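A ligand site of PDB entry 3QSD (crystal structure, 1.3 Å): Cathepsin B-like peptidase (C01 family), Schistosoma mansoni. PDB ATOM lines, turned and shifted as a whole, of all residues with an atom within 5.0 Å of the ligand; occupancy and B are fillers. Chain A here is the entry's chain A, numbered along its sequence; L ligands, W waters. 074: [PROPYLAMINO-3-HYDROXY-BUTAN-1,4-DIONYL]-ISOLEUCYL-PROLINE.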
ATOM      1  N   GLN A  25      10.495  -9.390 -22.866  1.00  0.00           N
ATOM      2  CA  GLN A  25       9.739  -8.146 -22.695  1.00  0.00           C
ATOM      3  C   GLN A  25       8.635  -7.943 -23.740  1.00  0.00           C
ATOM      4  O   GLN A  25       7.823  -7.009 -23.603  1.00  0.00           O
ATOM      5  CB  GLN A  25      10.668  -6.932 -22.713  1.00  0.00           C
ATOM      6  CG  GLN A  25      11.342  -6.745 -24.079  1.00  0.00           C
ATOM      7  CD  GLN A  25      12.406  -5.670 -24.008  1.00  0.00           C
ATOM      8  OE1 GLN A  25      13.533  -5.904 -23.571  1.00  0.00           O
ATOM      9  NE2 GLN A  25      12.068  -4.481 -24.496  1.00  0.00           N
ATOM     10  N   SER A  26       8.604  -8.776 -24.768  1.00  0.00           N
ATOM     11  CA  SER A  26       7.589  -8.685 -25.829  1.00  0.00           C
ATOM     12  C   SER A  26       7.677  -7.348 -26.601  1.00  0.00           C
ATOM     13  O   SER A  26       8.764  -6.736 -26.652  1.00  0.00           O
ATOM     14  CB  SER A  26       6.190  -8.985 -25.265  1.00  0.00           C
ATOM     15  OG  SER A  26       5.207  -9.158 -26.275  1.00  0.00           O
ATOM     16  N   ARG A  27       6.565  -6.929 -27.191  1.00  0.00           N
ATOM     17  CA  ARG A  27       6.513  -5.751 -28.067  1.00  0.00           C
ATOM     18  C   ARG A  27       6.327  -4.479 -27.264  1.00  0.00           C
ATOM     19  O   ARG A  27       5.305  -3.784 -27.366  1.00  0.00           O
ATOM     20  CB  ARG A  27       5.336  -5.899 -29.035  1.00  0.00           C
ATOM     21  CG  ARG A  27       5.460  -7.195 -29.886  1.00  0.00           C
ATOM     22  CD  ARG A  27       4.216  -7.302 -30.820  1.00  0.00           C
ATOM     23  NE  ARG A  27       4.372  -8.492 -31.642  1.00  0.00           N
ATOM     24  CZ  ARG A  27       4.077  -9.740 -31.265  1.00  0.00           C
ATOM     25  NH1 ARG A  27       3.481  -9.971 -30.071  1.00  0.00           N
ATOM     26  NH2 ARG A  27       4.398 -10.759 -32.054  1.00  0.00           N
ATOM     27  N   CYS A  28       7.283  -4.221 -26.399  1.00  0.00           N
ATOM     28  CA  CYS A  28       7.149  -3.128 -25.436  1.00  0.00           C
ATOM     29  C   CYS A  28       8.558  -2.701 -25.066  1.00  0.00           C
ATOM     30  O   CYS A  28       9.404  -3.575 -24.887  1.00  0.00           O
ATOM     31  CB  CYS A  28       6.418  -3.652 -24.196  1.00  0.00           C
ATOM     32  SG  CYS A  28       6.337  -2.565 -22.698  1.00  0.00           S
ATOM     33  N   GLY A  29       8.830  -1.398 -24.992  1.00  0.00           N
ATOM     34  CA  GLY A  29      10.163  -0.907 -24.639  1.00  0.00           C
ATOM     35  C   GLY A  29      10.377  -0.883 -23.134  1.00  0.00           C
ATOM     36  O   GLY A  29      10.755   0.140 -22.545  1.00  0.00           O
ATOM     37  N   SER A  30      10.152  -2.032 -22.492  1.00  0.00           N
ATOM     38  CA  SER A  30      10.230  -2.152 -21.052  1.00  0.00           C
ATOM     39  C   SER A  30      11.515  -2.804 -20.567  1.00  0.00           C
ATOM     40  O   SER A  30      11.554  -3.350 -19.443  1.00  0.00           O
ATOM     41  CB  SER A  30       9.001  -2.968 -20.545  1.00  0.00           C
ATOM     42  OG  SER A  30       8.945  -4.147 -21.335  1.00  0.00           O
ATOM     43  N   CYS A  31      12.589  -2.712 -21.350  1.00  0.00           N
ATOM     44  CA  CYS A  31      13.852  -3.305 -20.912  1.00  0.00           C
ATOM     45  C   CYS A  31      14.225  -2.800 -19.543  1.00  0.00           C
ATOM     46  O   CYS A  31      14.748  -3.556 -18.718  1.00  0.00           O
ATOM     47  CB  CYS A  31      14.962  -2.984 -21.951  1.00  0.00           C
ATOM     48  SG  CYS A  31      15.471  -1.255 -21.998  1.00  0.00           S
ATOM     49  N   TRP A  32      14.003  -1.526 -19.281  1.00  0.00           N
ATOM     50  CA  TRP A  32      14.333  -0.951 -17.965  1.00  0.00           C
ATOM     51  C   TRP A  32      13.684  -1.730 -16.799  1.00  0.00           C
ATOM     52  O   TRP A  32      14.326  -1.944 -15.755  1.00  0.00           O
ATOM     53  CB  TRP A  32      13.926   0.531 -17.901  1.00  0.00           C
ATOM     54  CG  TRP A  32      12.411   0.717 -18.037  1.00  0.00           C
ATOM     55  CD1 TRP A  32      11.667   0.855 -19.184  1.00  0.00           C
ATOM     56  CD2 TRP A  32      11.491   0.803 -16.937  1.00  0.00           C
ATOM     57  NE1 TRP A  32      10.325   1.013 -18.866  1.00  0.00           N
ATOM     58  CE2 TRP A  32      10.190   0.984 -17.492  1.00  0.00           C
ATOM     59  CE3 TRP A  32      11.649   0.749 -15.530  1.00  0.00           C
ATOM     60  CZ2 TRP A  32       9.069   1.118 -16.673  1.00  0.00           C
ATOM     61  CZ3 TRP A  32      10.543   0.841 -14.701  1.00  0.00           C
ATOM     62  CH2 TRP A  32       9.250   1.009 -15.288  1.00  0.00           C
ATOM     63  N   GLY A  74      10.039   3.285 -22.859  1.00  0.00           N
ATOM     64  CA  GLY A  74      11.376   3.437 -22.248  1.00  0.00           C
ATOM     65  C   GLY A  74      11.303   4.033 -20.866  1.00  0.00           C
ATOM     66  O   GLY A  74      10.348   4.748 -20.550  1.00  0.00           O
ATOM     67  N   GLY A  75      12.329   3.789 -20.048  1.00  0.00           N
ATOM     68  CA  GLY A  75      12.269   4.210 -18.641  1.00  0.00           C
ATOM     69  C   GLY A  75      13.651   4.567 -18.099  1.00  0.00           C
ATOM     70  O   GLY A  75      14.622   4.751 -18.865  1.00  0.00           O
ATOM     71  N   LEU A  77      16.480   3.957 -14.757  1.00  0.00           N
ATOM     72  CA  LEU A  77      16.877   2.883 -13.836  1.00  0.00           C
ATOM     73  C   LEU A  77      16.786   3.285 -12.376  1.00  0.00           C
ATOM     74  O   LEU A  77      16.244   2.550 -11.561  1.00  0.00           O
ATOM     75  CB  LEU A  77      18.319   2.466 -14.131  1.00  0.00           C
ATOM     76  CG  LEU A  77      18.530   1.330 -15.129  1.00  0.00           C
ATOM     77  CD1 LEU A  77      18.022   1.617 -16.523  1.00  0.00           C
ATOM     78  CD2 LEU A  77      19.993   0.934 -15.123  1.00  0.00           C
ATOM     79  N   HIS A 111      12.885 -11.231 -31.337  1.00  0.00           N
ATOM     80  CA  HIS A 111      13.462  -9.911 -31.362  1.00  0.00           C
ATOM     81  C   HIS A 111      14.656  -9.895 -32.331  1.00  0.00           C
ATOM     82  O   HIS A 111      15.774 -10.265 -31.966  1.00  0.00           O
ATOM     83  CB  HIS A 111      13.931  -9.499 -29.961  1.00  0.00           C
ATOM     84  CG  HIS A 111      12.827  -9.507 -28.949  1.00  0.00           C
ATOM     85  ND1 HIS A 111      12.219  -8.345 -28.544  1.00  0.00           N
ATOM     86  CD2 HIS A 111      12.248 -10.517 -28.234  1.00  0.00           C
ATOM     87  CE1 HIS A 111      11.306  -8.631 -27.616  1.00  0.00           C
ATOM     88  NE2 HIS A 111      11.284  -9.946 -27.420  1.00  0.00           N
ATOM     89  N   HIS A 112      14.426  -9.502 -33.587  1.00  0.00           N
ATOM     90  CA  HIS A 112      15.537  -9.274 -34.558  1.00  0.00           C
ATOM     91  C   HIS A 112      16.324 -10.538 -34.824  1.00  0.00           C
ATOM     92  O   HIS A 112      17.492 -10.444 -35.123  1.00  0.00           O
ATOM     93  CB  HIS A 112      16.500  -8.210 -34.002  1.00  0.00           C
ATOM     94  CG  HIS A 112      15.795  -7.012 -33.449  1.00  0.00           C
ATOM     95  ND1 HIS A 112      15.201  -6.060 -34.262  1.00  0.00           N
ATOM     96  CD2 HIS A 112      15.547  -6.608 -32.157  1.00  0.00           C
ATOM     97  CE1 HIS A 112      14.650  -5.112 -33.517  1.00  0.00           C
ATOM     98  NE2 HIS A 112      14.839  -5.419 -32.244  1.00  0.00           N
ATOM     99  N   CYS A 120       8.485 -10.250 -33.402  1.00  0.00           N
ATOM    100  CA  CYS A 120       7.966  -9.084 -32.670  1.00  0.00           C
ATOM    101  C   CYS A 120       7.425  -8.012 -33.604  1.00  0.00           C
ATOM    102  O   CYS A 120       6.499  -7.291 -33.266  1.00  0.00           O
ATOM    103  CB  CYS A 120       8.996  -8.462 -31.718  1.00  0.00           C
ATOM    104  SG  CYS A 120       9.524  -9.583 -30.400  1.00  0.00           S
ATOM    105  N   ILE A 124       4.404  -1.388 -31.114  1.00  0.00           N
ATOM    106  CA  ILE A 124       4.663  -1.399 -29.682  1.00  0.00           C
ATOM    107  C   ILE A 124       3.326  -1.311 -28.944  1.00  0.00           C
ATOM    108  O   ILE A 124       2.445  -0.495 -29.303  1.00  0.00           O
ATOM    109  CB  ILE A 124       5.507  -0.130 -29.315  1.00  0.00           C
ATOM    110  CG1 ILE A 124       6.829  -0.039 -30.123  1.00  0.00           C
ATOM    111  CG2 ILE A 124       5.866  -0.115 -27.851  1.00  0.00           C
ATOM    112  CD1 ILE A 124       7.855  -1.121 -29.801  1.00  0.00           C
ATOM    113  N   GLY A 175      22.709  -0.089 -17.830  1.00  0.00           N
ATOM    114  CA  GLY A 175      22.382   0.485 -19.115  1.00  0.00           C
ATOM    115  C   GLY A 175      23.558   0.526 -20.053  1.00  0.00           C
ATOM    116  O   GLY A 175      24.719   0.529 -19.637  1.00  0.00           O
ATOM    117  N   VAL A 178      22.618   1.171 -27.273  1.00  0.00           N
ATOM    118  CA  VAL A 178      22.305   0.147 -28.249  1.00  0.00           C
ATOM    119  C   VAL A 178      22.420   0.726 -29.659  1.00  0.00           C
ATOM    120  O   VAL A 178      21.678   1.638 -30.016  1.00  0.00           O
ATOM    121  CB  VAL A 178      20.930  -0.522 -27.977  1.00  0.00           C
ATOM    122  CG1 VAL A 178      19.742   0.511 -27.813  1.00  0.00           C
ATOM    123  CG2 VAL A 178      20.665  -1.588 -29.047  1.00  0.00           C
ATOM    124  N   LEU A 183      21.446  -5.503 -32.807  1.00  0.00           N
ATOM    125  CA  LEU A 183      20.222  -6.305 -33.178  1.00  0.00           C
ATOM    126  C   LEU A 183      20.542  -7.421 -34.181  1.00  0.00           C
ATOM    127  O   LEU A 183      19.748  -8.250 -34.626  1.00  0.00           O
ATOM    128  CB  LEU A 183      19.146  -5.426 -33.803  1.00  0.00           C
ATOM    129  CG  LEU A 183      18.893  -3.983 -33.342  1.00  0.00           C
ATOM    130  CD1 LEU A 183      17.687  -3.323 -34.029  1.00  0.00           C
ATOM    131  CD2 LEU A 183      18.814  -3.836 -31.839  1.00  0.00           C
ATOM    132  N   LEU A 198      20.358   3.510 -31.455  1.00  0.00           N
ATOM    133  CA  LEU A 198      18.936   3.319 -31.295  1.00  0.00           C
ATOM    134  C   LEU A 198      18.521   3.722 -29.882  1.00  0.00           C
ATOM    135  O   LEU A 198      17.392   3.470 -29.484  1.00  0.00           O
ATOM    136  CB  LEU A 198      18.608   1.847 -31.536  1.00  0.00           C
ATOM    137  CG  LEU A 198      18.875   1.384 -32.972  1.00  0.00           C
ATOM    138  CD1 LEU A 198      18.591  -0.090 -33.070  1.00  0.00           C
ATOM    139  CD2 LEU A 198      17.944   2.140 -33.947  1.00  0.00           C
ATOM    140  N   GLY A 200      19.134   3.915 -25.549  1.00  0.00           N
ATOM    141  CA  GLY A 200      19.647   3.157 -24.437  1.00  0.00           C
ATOM    142  C   GLY A 200      18.917   1.849 -24.256  1.00  0.00           C
ATOM    143  O   GLY A 200      17.717   1.712 -24.529  1.00  0.00           O
ATOM    144  N   HIS A 201      19.646   0.867 -23.755  1.00  0.00           N
ATOM    145  CA  HIS A 201      19.060  -0.447 -23.446  1.00  0.00           C
ATOM    146  C   HIS A 201      19.492  -0.824 -22.025  1.00  0.00           C
ATOM    147  O   HIS A 201      20.523  -0.356 -21.560  1.00  0.00           O
ATOM    148  CB  HIS A 201      19.549  -1.488 -24.439  1.00  0.00           C
ATOM    149  CG  HIS A 201      18.747  -2.743 -24.465  1.00  0.00           C
ATOM    150  ND1 HIS A 201      17.378  -2.737 -24.692  1.00  0.00           N
ATOM    151  CD2 HIS A 201      19.114  -4.044 -24.331  1.00  0.00           C
ATOM    152  CE1 HIS A 201      16.934  -3.990 -24.629  1.00  0.00           C
ATOM    153  NE2 HIS A 201      17.979  -4.811 -24.432  1.00  0.00           N
ATOM    154  N   ALA A 202      18.747  -1.642 -21.328  1.00  0.00           N
ATOM    155  CA  ALA A 202      19.029  -2.013 -19.953  1.00  0.00           C
ATOM    156  C   ALA A 202      18.928  -3.501 -19.856  1.00  0.00           C
ATOM    157  O   ALA A 202      17.976  -4.118 -20.376  1.00  0.00           O
ATOM    158  CB  ALA A 202      17.994  -1.397 -19.016  1.00  0.00           C
ATOM    159  N   TRP A 223      15.061 -10.735 -24.271  1.00  0.00           N
ATOM    160  CA  TRP A 223      14.522 -10.964 -25.611  1.00  0.00           C
ATOM    161  C   TRP A 223      14.306 -12.467 -25.848  1.00  0.00           C
ATOM    162  O   TRP A 223      14.340 -12.941 -26.988  1.00  0.00           O
ATOM    163  CB  TRP A 223      15.468 -10.387 -26.669  1.00  0.00           C
ATOM    164  CG  TRP A 223      15.458  -8.892 -26.749  1.00  0.00           C
ATOM    165  CD1 TRP A 223      14.696  -8.024 -26.008  1.00  0.00           C
ATOM    166  CD2 TRP A 223      16.258  -8.091 -27.608  1.00  0.00           C
ATOM    167  NE1 TRP A 223      14.970  -6.729 -26.384  1.00  0.00           N
ATOM    168  CE2 TRP A 223      15.938  -6.751 -27.366  1.00  0.00           C
ATOM    169  CE3 TRP A 223      17.252  -8.384 -28.558  1.00  0.00           C
ATOM    170  CZ2 TRP A 223      16.555  -5.689 -28.025  1.00  0.00           C
ATOM    171  CZ3 TRP A 223      17.857  -7.350 -29.236  1.00  0.00           C
ATOM    172  CH2 TRP A 223      17.553  -6.013 -28.942  1.00  0.00           C
ATOM    173  N   GLU A 247      26.496   2.914 -16.200  1.00  0.00           N
ATOM    174  CA  GLU A 247      25.061   3.026 -15.909  1.00  0.00           C
ATOM    175  C   GLU A 247      24.599   1.838 -15.071  1.00  0.00           C
ATOM    176  O   GLU A 247      23.510   1.282 -15.312  1.00  0.00           O
ATOM    177  CB  GLU A 247      24.264   3.040 -17.217  1.00  0.00           C
ATOM    178  CG  GLU A 247      24.682   4.129 -18.205  1.00  0.00           C
ATOM    179  CD  GLU A 247      24.001   4.025 -19.537  1.00  0.00           C
ATOM    180  OE1 GLU A 247      22.759   3.974 -19.554  1.00  0.00           O
ATOM    181  OE2 GLU A 247      24.754   3.938 -20.516  1.00  0.00           O
HETATM  182  C1  074 L   1      18.213   3.007 -19.288  1.00  0.00           C
HETATM  183  C2  074 L   1      17.418   2.195 -20.283  1.00  0.00           C
HETATM  184  C3  074 L   1      16.582   3.054 -21.195  1.00  0.00           C
HETATM  185  N1  074 L   1      15.944   2.223 -22.254  1.00  0.00           N
HETATM  186  C4  074 L   1      14.771   1.600 -22.088  1.00  0.00           C
HETATM  187  O1  074 L   1      14.120   1.735 -21.018  1.00  0.00           O
HETATM  188  C5  074 L   1      14.141   0.816 -23.189  1.00  0.00           C
HETATM  189  O2  074 L   1      14.123   1.668 -24.354  1.00  0.00           O
HETATM  190  C6  074 L   1      14.997  -0.416 -23.573  1.00  0.00           C
HETATM  191  C7  074 L   1      14.159  -1.193 -24.518  1.00  0.00           C
HETATM  192  O3  074 L   1      13.107  -1.767 -24.201  1.00  0.00           O
HETATM  193  N2  074 L   1      14.586  -1.121 -25.771  1.00  0.00           N
HETATM  194  C8  074 L   1      13.787  -1.528 -26.889  1.00  0.00           C
HETATM  195  C13 074 L   1      13.547  -2.984 -27.067  1.00  0.00           C
HETATM  196  O4  074 L   1      14.365  -3.777 -26.613  1.00  0.00           O
HETATM  197  C9  074 L   1      14.452  -0.946 -28.216  1.00  0.00           C
HETATM  198  C11 074 L   1      15.870  -1.504 -28.382  1.00  0.00           C
HETATM  199  C10 074 L   1      14.395   0.614 -28.144  1.00  0.00           C
HETATM  200  C12 074 L   1      16.347  -1.222 -29.798  1.00  0.00           C
HETATM  201  N3  074 L   1      12.460  -3.325 -27.738  1.00  0.00           N
HETATM  202  C17 074 L   1      12.263  -4.709 -28.106  1.00  0.00           C
HETATM  203  C18 074 L   1      13.078  -5.021 -29.388  1.00  0.00           C
HETATM  204  O   074 L   1      13.670  -4.105 -30.063  1.00  0.00           O
HETATM  205  C16 074 L   1      10.804  -4.801 -28.489  1.00  0.00           C
HETATM  206  C15 074 L   1      10.494  -3.404 -28.963  1.00  0.00           C
HETATM  207  C14 074 L   1      11.395  -2.444 -28.221  1.00  0.00           C
HETATM  208  OT  074 L   1      13.115  -6.206 -29.794  1.00  0.00           O
HETATM  209  O   HOH W   1      11.872   2.132 -25.748  1.00  0.00           O
HETATM  210  O   HOH W   2      20.715   4.409 -17.340  1.00  0.00           O
HETATM  211  O   HOH W   3      11.674  -6.529 -32.146  1.00  0.00           O
HETATM  212  O   HOH W   4      14.622   4.714 -23.930  1.00  0.00           O
HETATM  213  O   HOH W   5      12.954  -1.864 -31.494  1.00  0.00           O
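N of Cys 31 sits at hydrogen-bond distance from O3 of the ligand (3.0 Å).
The side-chain sulfur of Cys 31 is bonded to a carbon (C6) of the ligand, 1.8 Å away.
ND1 of His 111 is in hydrogen-bond range of OT of the ligand (2.6 Å).
O of the ligand lies within hydrogen-bond range of NE2 of His 112.
N of Gly 75 lies within hydrogen-bond range of O1 of the ligand (2.9 Å).
An oxygen (O3) of the ligand lies within hydrogen-bond range of the side-chain amide nitrogen (NE2) of Gln 25 (2.9 Å).
O of Gly 200 is in hydrogen-bond range of N1 of the ligand, 2.9 Å away.
O4 of the ligand lies within hydrogen-bond range of NE1 of Trp 223, 3.0 Å away.
N2 of the ligand lies within hydrogen-bond range of ND1 of His 201.
The backbone NH of Ser 30 sits at hydrogen-bond distance from an oxygen (O3) of the ligand, 3.4 Å away.
SG of Cys 31 is in hydrogen-bond range of ND1 of His 201, at 3.6 Å.
The side-chain sulfur (SG) of Cys 31 lies within hydrogen-bond range of the backbone NH (N) of Ala 202 (3.4 Å).
NE2 of His 111 sits close to SG of Cys 120 (3.5 Å).
OE1 of Gln 25 sits at hydrogen-bond distance from NE1 of Trp 223, at 3.3 Å.
The side-chain amide nitrogen of Gln 25 lies within hydrogen-bond range of the backbone carbonyl oxygen of Cys 28, at 2.8 Å.
The backbone carbonyl oxygen (O) of Gly 29 lies within hydrogen-bond range of the backbone NH (N) of Gly 74, 3.2 Å away.
The side-chain hydroxyl (OG) of Ser 30 sits at hydrogen-bond distance from the side-chain sulfur (SG) of Cys 28 (3.3 Å).
O of Gly 29 lies close to O3 of the ligand (3.5 Å).
Merely in contact with the ligand: Ser 26 (3.4 Å), Trp 32 (3.2 Å), Gly 74 (3.5 Å), Leu 77 (3.1 Å), Ile 124 (3.6 Å) and Ala 202 (3.9 Å).
Hydrophobic or aromatic side chains within 4 Å of the ligand: Trp 32, Leu 77, His 111, His 112, Ile 124, His 201, Ala 202 and Trp 223.
16 residues have an atom within 4 Å of the ligand: Gln 25, Ser 26, Gly 29, Ser 30, Cys 31, Trp 32, Gly 74, Gly 75, Leu 77, His 111, His 112, Ile 124, Gly 200, His 201, Ala 202 and Trp 223.
Water W3 bridges OT of the ligand (2.8 Å) and NE2 of His 112 (3.4 Å).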
